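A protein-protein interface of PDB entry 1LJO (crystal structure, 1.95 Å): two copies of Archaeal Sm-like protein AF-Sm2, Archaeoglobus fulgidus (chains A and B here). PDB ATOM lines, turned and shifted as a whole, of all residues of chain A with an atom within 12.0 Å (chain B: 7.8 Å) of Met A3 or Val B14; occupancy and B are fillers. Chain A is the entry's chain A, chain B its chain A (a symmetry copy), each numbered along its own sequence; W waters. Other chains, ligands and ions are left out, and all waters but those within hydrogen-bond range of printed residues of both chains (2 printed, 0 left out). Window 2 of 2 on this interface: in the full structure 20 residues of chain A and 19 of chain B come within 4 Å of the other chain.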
ATOM      1  N   GLY A   1      16.632 -36.076 -28.852  1.00  0.00           N
ATOM      2  CA  GLY A   1      17.949 -35.379 -28.851  1.00  0.00           C
ATOM      3  C   GLY A   1      18.224 -34.650 -27.550  1.00  0.00           C
ATOM      4  O   GLY A   1      18.448 -35.279 -26.515  1.00  0.00           O
ATOM      5  N   ALA A   2      18.206 -33.322 -27.601  1.00  0.00           N
ATOM      6  CA  ALA A   2      18.453 -32.500 -26.423  1.00  0.00           C
ATOM      7  C   ALA A   2      17.613 -31.231 -26.462  1.00  0.00           C
ATOM      8  O   ALA A   2      17.098 -30.844 -27.516  1.00  0.00           O
ATOM      9  CB  ALA A   2      19.930 -32.140 -26.337  1.00  0.00           C
ATOM     10  N   MET A   3      17.471 -30.586 -25.310  1.00  0.00           N
ATOM     11  CA  MET A   3      16.703 -29.354 -25.230  1.00  0.00           C
ATOM     12  C   MET A   3      17.124 -28.548 -24.013  1.00  0.00           C
ATOM     13  O   MET A   3      17.694 -29.088 -23.067  1.00  0.00           O
ATOM     14  CB  MET A   3      15.200 -29.654 -25.164  1.00  0.00           C
ATOM     15  CG  MET A   3      14.712 -30.263 -23.858  1.00  0.00           C
ATOM     16  SD  MET A   3      12.902 -30.352 -23.809  1.00  0.00           S
ATOM     17  CE  MET A   3      12.633 -31.771 -22.742  1.00  0.00           C
ATOM     18  N   VAL A   4      16.849 -27.249 -24.051  1.00  0.00           N
ATOM     19  CA  VAL A   4      17.193 -26.359 -22.949  1.00  0.00           C
ATOM     20  C   VAL A   4      15.939 -26.041 -22.144  1.00  0.00           C
ATOM     21  O   VAL A   4      14.976 -25.488 -22.677  1.00  0.00           O
ATOM     22  CB  VAL A   4      17.806 -25.041 -23.473  1.00  0.00           C
ATOM     23  CG1 VAL A   4      18.215 -24.150 -22.308  1.00  0.00           C
ATOM     24  CG2 VAL A   4      19.006 -25.348 -24.351  1.00  0.00           C
ATOM     25  N   LEU A   5      15.949 -26.400 -20.865  1.00  0.00           N
ATOM     26  CA  LEU A   5      14.802 -26.149 -20.001  1.00  0.00           C
ATOM     27  C   LEU A   5      14.574 -24.656 -19.786  1.00  0.00           C
ATOM     28  O   LEU A   5      15.521 -23.884 -19.652  1.00  0.00           O
ATOM     29  CB  LEU A   5      14.993 -26.837 -18.649  1.00  0.00           C
ATOM     30  CG  LEU A   5      14.970 -28.370 -18.676  1.00  0.00           C
ATOM     31  CD1 LEU A   5      15.376 -28.919 -17.315  1.00  0.00           C
ATOM     32  CD2 LEU A   5      13.577 -28.855 -19.064  1.00  0.00           C
ATOM     33  N   PRO A   6      13.304 -24.227 -19.778  1.00  0.00           N
ATOM     34  CA  PRO A   6      12.997 -22.812 -19.571  1.00  0.00           C
ATOM     35  C   PRO A   6      13.668 -22.253 -18.311  1.00  0.00           C
ATOM     36  O   PRO A   6      14.281 -21.191 -18.355  1.00  0.00           O
ATOM     37  CB  PRO A   6      11.476 -22.810 -19.489  1.00  0.00           C
ATOM     38  CG  PRO A   6      11.111 -23.868 -20.494  1.00  0.00           C
ATOM     39  CD  PRO A   6      12.087 -24.980 -20.138  1.00  0.00           C
ATOM     40  N   ASN A   7      13.560 -22.967 -17.193  1.00  0.00           N
ATOM     41  CA  ASN A   7      14.186 -22.511 -15.951  1.00  0.00           C
ATOM     42  C   ASN A   7      15.696 -22.369 -16.126  1.00  0.00           C
ATOM     43  O   ASN A   7      16.310 -21.480 -15.534  1.00  0.00           O
ATOM     44  CB  ASN A   7      13.895 -23.480 -14.798  1.00  0.00           C
ATOM     45  CG  ASN A   7      12.497 -23.311 -14.226  1.00  0.00           C
ATOM     46  OD1 ASN A   7      12.063 -24.096 -13.383  1.00  0.00           O
ATOM     47  ND2 ASN A   7      11.791 -22.283 -14.675  1.00  0.00           N
ATOM     48  N   GLN A   8      16.295 -23.247 -16.928  1.00  0.00           N
ATOM     49  CA  GLN A   8      17.736 -23.185 -17.174  1.00  0.00           C
ATOM     50  C   GLN A   8      18.041 -21.899 -17.936  1.00  0.00           C
ATOM     51  O   GLN A   8      19.008 -21.196 -17.642  1.00  0.00           O
ATOM     52  CB  GLN A   8      18.213 -24.378 -18.021  1.00  0.00           C
ATOM     53  CG  GLN A   8      18.115 -25.746 -17.357  1.00  0.00           C
ATOM     54  CD  GLN A   8      18.768 -26.849 -18.191  1.00  0.00           C
ATOM     55  OE1 GLN A   8      18.392 -27.088 -19.341  1.00  0.00           O
ATOM     56  NE2 GLN A   8      19.749 -27.526 -17.606  1.00  0.00           N
ATOM     57  N   MET A   9      17.210 -21.605 -18.929  1.00  0.00           N
ATOM     58  CA  MET A   9      17.393 -20.410 -19.739  1.00  0.00           C
ATOM     59  C   MET A   9      17.265 -19.148 -18.884  1.00  0.00           C
ATOM     60  O   MET A   9      18.119 -18.265 -18.944  1.00  0.00           O
ATOM     61  CB  MET A   9      16.369 -20.385 -20.882  1.00  0.00           C
ATOM     62  CG  MET A   9      16.533 -19.217 -21.847  1.00  0.00           C
ATOM     63  SD  MET A   9      18.203 -19.121 -22.553  1.00  0.00           S
ATOM     64  CE  MET A   9      18.201 -17.455 -23.186  1.00  0.00           C
ATOM     65  N   VAL A  10      16.213 -19.070 -18.076  1.00  0.00           N
ATOM     66  CA  VAL A  10      16.006 -17.894 -17.235  1.00  0.00           C
ATOM     67  C   VAL A  10      17.153 -17.680 -16.254  1.00  0.00           C
ATOM     68  O   VAL A  10      17.579 -16.547 -16.032  1.00  0.00           O
ATOM     69  CB  VAL A  10      14.673 -17.980 -16.447  1.00  0.00           C
ATOM     70  CG1 VAL A  10      14.513 -16.753 -15.550  1.00  0.00           C
ATOM     71  CG2 VAL A  10      13.499 -18.078 -17.414  1.00  0.00           C
ATOM     72  N   SER A  12      20.195 -18.460 -16.686  1.00  0.00           N
ATOM     73  CA  SER A  12      21.356 -17.994 -17.435  1.00  0.00           C
ATOM     74  C   SER A  12      21.287 -16.485 -17.680  1.00  0.00           C
ATOM     75  O   SER A  12      22.288 -15.866 -18.023  1.00  0.00           O
ATOM     76  CB  SER A  12      21.459 -18.723 -18.780  1.00  0.00           C
ATOM     77  OG  SER A  12      20.480 -18.271 -19.698  1.00  0.00           O
ATOM     78  N   ASN B   7       1.386 -33.203 -22.229  1.00  0.00           N
ATOM     79  CA  ASN B   7       2.823 -32.992 -22.049  1.00  0.00           C
ATOM     80  C   ASN B   7       3.622 -33.810 -23.062  1.00  0.00           C
ATOM     81  O   ASN B   7       4.676 -33.370 -23.523  1.00  0.00           O
ATOM     82  CB  ASN B   7       3.263 -33.370 -20.629  1.00  0.00           C
ATOM     83  CG  ASN B   7       2.916 -32.305 -19.602  1.00  0.00           C
ATOM     84  OD1 ASN B   7       3.086 -32.510 -18.401  1.00  0.00           O
ATOM     85  ND2 ASN B   7       2.438 -31.160 -20.072  1.00  0.00           N
ATOM     86  N   GLN B   8       3.127 -34.999 -23.399  1.00  0.00           N
ATOM     87  CA  GLN B   8       3.808 -35.851 -24.376  1.00  0.00           C
ATOM     88  C   GLN B   8       3.761 -35.162 -25.736  1.00  0.00           C
ATOM     89  O   GLN B   8       4.747 -35.132 -26.472  1.00  0.00           O
ATOM     90  CB  GLN B   8       3.122 -37.223 -24.500  1.00  0.00           C
ATOM     91  CG  GLN B   8       3.196 -38.117 -23.269  1.00  0.00           C
ATOM     92  CD  GLN B   8       2.647 -39.520 -23.531  1.00  0.00           C
ATOM     93  OE1 GLN B   8       1.487 -39.692 -23.911  1.00  0.00           O
ATOM     94  NE2 GLN B   8       3.487 -40.528 -23.322  1.00  0.00           N
ATOM     95  N   MET B   9       2.596 -34.617 -26.067  1.00  0.00           N
ATOM     96  CA  MET B   9       2.415 -33.936 -27.340  1.00  0.00           C
ATOM     97  C   MET B   9       3.332 -32.716 -27.440  1.00  0.00           C
ATOM     98  O   MET B   9       4.032 -32.542 -28.436  1.00  0.00           O
ATOM     99  CB  MET B   9       0.949 -33.514 -27.510  1.00  0.00           C
ATOM    100  CG  MET B   9       0.631 -32.871 -28.854  1.00  0.00           C
ATOM    101  SD  MET B   9       1.109 -33.915 -30.260  1.00  0.00           S
ATOM    102  CE  MET B   9       1.080 -32.723 -31.585  1.00  0.00           C
ATOM    103  N   VAL B  10       3.345 -31.884 -26.404  1.00  0.00           N
ATOM    104  CA  VAL B  10       4.183 -30.686 -26.421  1.00  0.00           C
ATOM    105  C   VAL B  10       5.664 -31.023 -26.553  1.00  0.00           C
ATOM    106  O   VAL B  10       6.393 -30.347 -27.278  1.00  0.00           O
ATOM    107  CB  VAL B  10       3.970 -29.820 -25.153  1.00  0.00           C
ATOM    108  CG1 VAL B  10       4.890 -28.601 -25.189  1.00  0.00           C
ATOM    109  CG2 VAL B  10       2.515 -29.374 -25.061  1.00  0.00           C
ATOM    110  N   LYS B  11       6.111 -32.068 -25.863  1.00  0.00           N
ATOM    111  CA  LYS B  11       7.514 -32.443 -25.944  1.00  0.00           C
ATOM    112  C   LYS B  11       7.870 -32.897 -27.357  1.00  0.00           C
ATOM    113  O   LYS B  11       8.982 -32.672 -27.820  1.00  0.00           O
ATOM    114  CB  LYS B  11       7.846 -33.547 -24.930  1.00  0.00           C
ATOM    115  CG  LYS B  11       9.341 -33.837 -24.818  1.00  0.00           C
ATOM    116  CD  LYS B  11       9.675 -34.745 -23.637  1.00  0.00           C
ATOM    117  CE  LYS B  11       9.093 -36.142 -23.805  1.00  0.00           C
ATOM    118  NZ  LYS B  11       9.648 -36.843 -24.998  1.00  0.00           N
ATOM    119  N   SER B  12       6.921 -33.519 -28.049  1.00  0.00           N
ATOM    120  CA  SER B  12       7.164 -33.979 -29.410  1.00  0.00           C
ATOM    121  C   SER B  12       7.349 -32.799 -30.368  1.00  0.00           C
ATOM    122  O   SER B  12       7.849 -32.970 -31.474  1.00  0.00           O
ATOM    123  CB  SER B  12       6.006 -34.856 -29.901  1.00  0.00           C
ATOM    124  OG  SER B  12       4.854 -34.085 -30.193  1.00  0.00           O
ATOM    125  N   MET B  13       6.948 -31.607 -29.934  1.00  0.00           N
ATOM    126  CA  MET B  13       7.079 -30.404 -30.760  1.00  0.00           C
ATOM    127  C   MET B  13       8.455 -29.750 -30.632  1.00  0.00           C
ATOM    128  O   MET B  13       8.756 -28.785 -31.337  1.00  0.00           O
ATOM    129  CB  MET B  13       6.007 -29.377 -30.382  1.00  0.00           C
ATOM    130  CG  MET B  13       4.589 -29.734 -30.790  1.00  0.00           C
ATOM    131  SD  MET B  13       3.402 -28.470 -30.236  1.00  0.00           S
ATOM    132  CE  MET B  13       2.483 -29.385 -29.023  1.00  0.00           C
ATOM    133  N   VAL B  14       9.286 -30.263 -29.728  1.00  0.00           N
ATOM    134  CA  VAL B  14      10.616 -29.696 -29.535  1.00  0.00           C
ATOM    135  C   VAL B  14      11.434 -29.803 -30.815  1.00  0.00           C
ATOM    136  O   VAL B  14      11.434 -30.837 -31.482  1.00  0.00           O
ATOM    137  CB  VAL B  14      11.373 -30.404 -28.394  1.00  0.00           C
ATOM    138  CG1 VAL B  14      12.836 -29.987 -28.401  1.00  0.00           C
ATOM    139  CG2 VAL B  14      10.735 -30.053 -27.058  1.00  0.00           C
ATOM    140  N   GLY B  15      12.135 -28.730 -31.154  1.00  0.00           N
ATOM    141  CA  GLY B  15      12.932 -28.735 -32.366  1.00  0.00           C
ATOM    142  C   GLY B  15      12.129 -28.283 -33.575  1.00  0.00           C
ATOM    143  O   GLY B  15      12.674 -28.091 -34.655  1.00  0.00           O
ATOM    144  N   LYS B  16      10.828 -28.100 -33.392  1.00  0.00           N
ATOM    145  CA  LYS B  16       9.967 -27.675 -34.489  1.00  0.00           C
ATOM    146  C   LYS B  16       9.339 -26.313 -34.226  1.00  0.00           C
ATOM    147  O   LYS B  16       9.392 -25.805 -33.111  1.00  0.00           O
ATOM    148  CB  LYS B  16       8.876 -28.722 -34.731  1.00  0.00           C
ATOM    149  CG  LYS B  16       9.448 -30.116 -34.968  1.00  0.00           C
ATOM    150  CD  LYS B  16       8.403 -31.105 -35.459  1.00  0.00           C
ATOM    151  CE  LYS B  16       9.053 -32.447 -35.766  1.00  0.00           C
ATOM    152  NZ  LYS B  16       8.096 -33.418 -36.361  1.00  0.00           N
ATOM    153  N   ILE B  17       8.747 -25.735 -35.269  1.00  0.00           N
ATOM    154  CA  ILE B  17       8.100 -24.428 -35.194  1.00  0.00           C
ATOM    155  C   ILE B  17       6.680 -24.544 -34.652  1.00  0.00           C
ATOM    156  O   ILE B  17       5.888 -25.355 -35.132  1.00  0.00           O
ATOM    157  CB  ILE B  17       7.998 -23.767 -36.588  1.00  0.00           C
ATOM    158  CG1 ILE B  17       9.373 -23.728 -37.260  1.00  0.00           C
ATOM    159  CG2 ILE B  17       7.406 -22.365 -36.457  1.00  0.00           C
ATOM    160  CD1 ILE B  17      10.426 -22.993 -36.467  1.00  0.00           C
ATOM    161  N   ILE B  18       6.358 -23.719 -33.661  1.00  0.00           N
ATOM    162  CA  ILE B  18       5.028 -23.738 -33.070  1.00  0.00           C
ATOM    163  C   ILE B  18       4.463 -22.327 -32.984  1.00  0.00           C
ATOM    164  O   ILE B  18       5.208 -21.349 -33.062  1.00  0.00           O
ATOM    165  CB  ILE B  18       5.048 -24.346 -31.646  1.00  0.00           C
ATOM    166  CG1 ILE B  18       5.864 -23.458 -30.699  1.00  0.00           C
ATOM    167  CG2 ILE B  18       5.666 -25.742 -31.687  1.00  0.00           C
ATOM    168  CD1 ILE B  18       5.752 -23.858 -29.224  1.00  0.00           C
ATOM    169  N   LYS B  32      10.834 -21.455 -32.822  1.00  0.00           N
ATOM    170  CA  LYS B  32      11.286 -22.828 -32.656  1.00  0.00           C
ATOM    171  C   LYS B  32      11.254 -23.196 -31.181  1.00  0.00           C
ATOM    172  O   LYS B  32      11.820 -22.489 -30.336  1.00  0.00           O
ATOM    173  CB  LYS B  32      12.710 -22.993 -33.195  1.00  0.00           C
ATOM    174  CG  LYS B  32      13.254 -24.422 -33.097  1.00  0.00           C
ATOM    175  CD  LYS B  32      14.750 -24.446 -33.385  1.00  0.00           C
ATOM    176  CE  LYS B  32      15.330 -25.839 -33.207  1.00  0.00           C
ATOM    177  NZ  LYS B  32      16.820 -25.811 -33.092  1.00  0.00           N
ATOM    178  N   LEU B  33      10.588 -24.306 -30.873  1.00  0.00           N
ATOM    179  CA  LEU B  33      10.499 -24.758 -29.494  1.00  0.00           C
ATOM    180  C   LEU B  33      11.810 -25.440 -29.123  1.00  0.00           C
ATOM    181  O   LEU B  33      12.098 -26.540 -29.588  1.00  0.00           O
ATOM    182  CB  LEU B  33       9.329 -25.736 -29.315  1.00  0.00           C
ATOM    183  CG  LEU B  33       9.135 -26.265 -27.886  1.00  0.00           C
ATOM    184  CD1 LEU B  33       8.910 -25.110 -26.929  1.00  0.00           C
ATOM    185  CD2 LEU B  33       7.956 -27.230 -27.852  1.00  0.00           C
ATOM    186  N   GLU B  34      12.604 -24.765 -28.297  1.00  0.00           N
ATOM    187  CA  GLU B  34      13.896 -25.289 -27.863  1.00  0.00           C
ATOM    188  C   GLU B  34      13.816 -26.013 -26.530  1.00  0.00           C
ATOM    189  O   GLU B  34      14.685 -26.819 -26.205  1.00  0.00           O
ATOM    190  CB  GLU B  34      14.916 -24.152 -27.763  1.00  0.00           C
ATOM    191  CG  GLU B  34      15.535 -23.783 -29.093  1.00  0.00           C
ATOM    192  CD  GLU B  34      16.507 -24.834 -29.581  1.00  0.00           C
ATOM    193  OE1 GLU B  34      17.590 -24.974 -28.974  1.00  0.00           O
ATOM    194  OE2 GLU B  34      16.182 -25.530 -30.564  1.00  0.00           O
ATOM    195  N   GLY B  35      12.776 -25.723 -25.757  1.00  0.00           N
ATOM    196  CA  GLY B  35      12.630 -26.374 -24.469  1.00  0.00           C
ATOM    197  C   GLY B  35      11.272 -26.162 -23.832  1.00  0.00           C
ATOM    198  O   GLY B  35      10.611 -25.152 -24.072  1.00  0.00           O
ATOM    199  N   VAL B  36      10.859 -27.126 -23.018  1.00  0.00           N
ATOM    200  CA  VAL B  36       9.583 -27.069 -22.324  1.00  0.00           C
ATOM    201  C   VAL B  36       9.677 -27.917 -21.053  1.00  0.00           C
ATOM    202  O   VAL B  36      10.500 -28.830 -20.980  1.00  0.00           O
ATOM    203  CB  VAL B  36       8.437 -27.613 -23.225  1.00  0.00           C
ATOM    204  CG1 VAL B  36       8.762 -29.026 -23.690  1.00  0.00           C
ATOM    205  CG2 VAL B  36       7.115 -27.597 -22.470  1.00  0.00           C
ATOM    206  N   ASP B  37       8.865 -27.595 -20.046  1.00  0.00           N
ATOM    207  CA  ASP B  37       8.851 -28.370 -18.803  1.00  0.00           C
ATOM    208  C   ASP B  37       7.431 -28.823 -18.481  1.00  0.00           C
ATOM    209  O   ASP B  37       6.496 -28.521 -19.225  1.00  0.00           O
ATOM    210  CB  ASP B  37       9.429 -27.570 -17.628  1.00  0.00           C
ATOM    211  CG  ASP B  37       8.760 -26.224 -17.442  1.00  0.00           C
ATOM    212  OD1 ASP B  37       7.540 -26.127 -17.675  1.00  0.00           O
ATOM    213  OD2 ASP B  37       9.463 -25.265 -17.045  1.00  0.00           O
ATOM    214  N   TYR B  43      10.412 -22.313 -24.045  1.00  0.00           N
ATOM    215  CA  TYR B  43      11.586 -21.560 -24.450  1.00  0.00           C
ATOM    216  C   TYR B  43      11.656 -21.640 -25.969  1.00  0.00           C
ATOM    217  O   TYR B  43      11.893 -22.707 -26.538  1.00  0.00           O
ATOM    218  CB  TYR B  43      12.863 -22.124 -23.816  1.00  0.00           C
ATOM    219  CG  TYR B  43      14.146 -21.538 -24.381  1.00  0.00           C
ATOM    220  CD1 TYR B  43      14.216 -20.201 -24.776  1.00  0.00           C
ATOM    221  CD2 TYR B  43      15.291 -22.319 -24.516  1.00  0.00           C
ATOM    222  CE1 TYR B  43      15.389 -19.659 -25.294  1.00  0.00           C
ATOM    223  CE2 TYR B  43      16.471 -21.788 -25.032  1.00  0.00           C
ATOM    224  CZ  TYR B  43      16.510 -20.458 -25.422  1.00  0.00           C
ATOM    225  OH  TYR B  43      17.662 -19.931 -25.962  1.00  0.00           O
HETATM  226  O   HOH W   1      15.892 -28.289 -28.750  1.00  0.00           O
HETATM  227  O   HOH W   2      12.163 -25.348 -16.757  1.00  0.00           O
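Among the printed residues, pairs that only touch across the chains: Met A3 with Val B14, Met A3 with Glu B34, Met A3 with Val B36, Val A4 with Gly B35, Val A4 with Tyr B43, Leu A5 with Val B36, Pro A6 with Gly B35, Pro A6 with Val B36 and Pro A6 with Tyr B43.
The side-chain amide oxygen of Gln A8 is in hydrogen-bond range of the backbone NH of Leu A5 (3.0 Å).
The backbone NH of Glu B34 is in hydrogen-bond range of the backbone carbonyl oxygen of Tyr B43 (2.8 Å).
The backbone carbonyl oxygen (O) of Gly B35 lies within hydrogen-bond range of the backbone NH (N) of Tyr B43, at 2.8 Å.
OE2 of Glu B34 lies within salt-bridge range of NZ of Lys B32, at 2.6 Å.
OG of Ser A12 is in hydrogen-bond range of O of Met A9 (2.5 Å).
Positions printed for both chains: 7, 8, 9, 10 and 12.
Of the 11 pairs that touch across the chains among the printed residues, none has its exchanged pair printed and touching as well.
Hydrophobic or aromatic side chains of chain B that line the printed part of chain A: Val B14 and Tyr B43.
Printed residues of chain A that touch a printed residue of chain B: Met A3, Val A4, Leu A5, Pro A6 and Met A9.
Hydrophobic or aromatic side chains of chain A within 4 Å of the printed part of chain B: Met A3, Val A4, Leu A5, Pro A6 and Met A9.
Among the printed residues, 11 pairs touch across the chains.
Among the printed residues, no Asp or Glu carboxylate lies within 4 Å of a Lys or Arg side-chain nitrogen of the other chain.
Water W2 bridges the side-chain carboxylate (OD2) of Asp B37 and the backbone NH (N) of Asn A7.
Water W1 lies within hydrogen-bond range of O of Ala A2 (3.1 Å) and O of Glu B34 (3.2 Å).
The side-chain hydroxyl (OH) of Tyr B43 sits at hydrogen-bond distance from the side-chain sulfur (SD) of Met A9.
N of Val A4 sits at hydrogen-bond distance from O of Glu B34.
Ala A2 touches none of the printed residues of chain B.
Of the printed residues of chain B, Pro A6 touches Gly B35 (3.8 Å), Val B36 (3.8 Å) and Tyr B43 (3.9 Å).
Printed residues of chain B within 4 Å of Met A9: Tyr B43 (3.5 Å).
No residue of chain A comes within 4 Å of Lys B11.
No residue of chain A comes within 4 Å of Met B13.
Val B14 touches just one residue of chain A: Met A3.
No residue of chain A comes within 4 Å of Gly B15.
Glu B34 touches just these residues of chain A: Met A3 (3.1 Å) and Val A4 (3.1 Å).
Of chain A, only Val A4 (3.1 Å) and Pro A6 (3.8 Å) come within 4 Å of Gly B35.
Of chain A, only Met A3 (3.9 Å), Leu A5 (3.6 Å) and Pro A6 (3.8 Å) come within 4 Å of Val B36.
Of the printed residues of chain A, Tyr B43 touches Val A4, Pro A6 and Met A9.
The nearest residue of chain B that does not touch Met A3 is Gly B35 (4.04 Å).
The nearest printed residue of chain B that does not touch Pro A6 is Asp B37 (4.01 Å).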
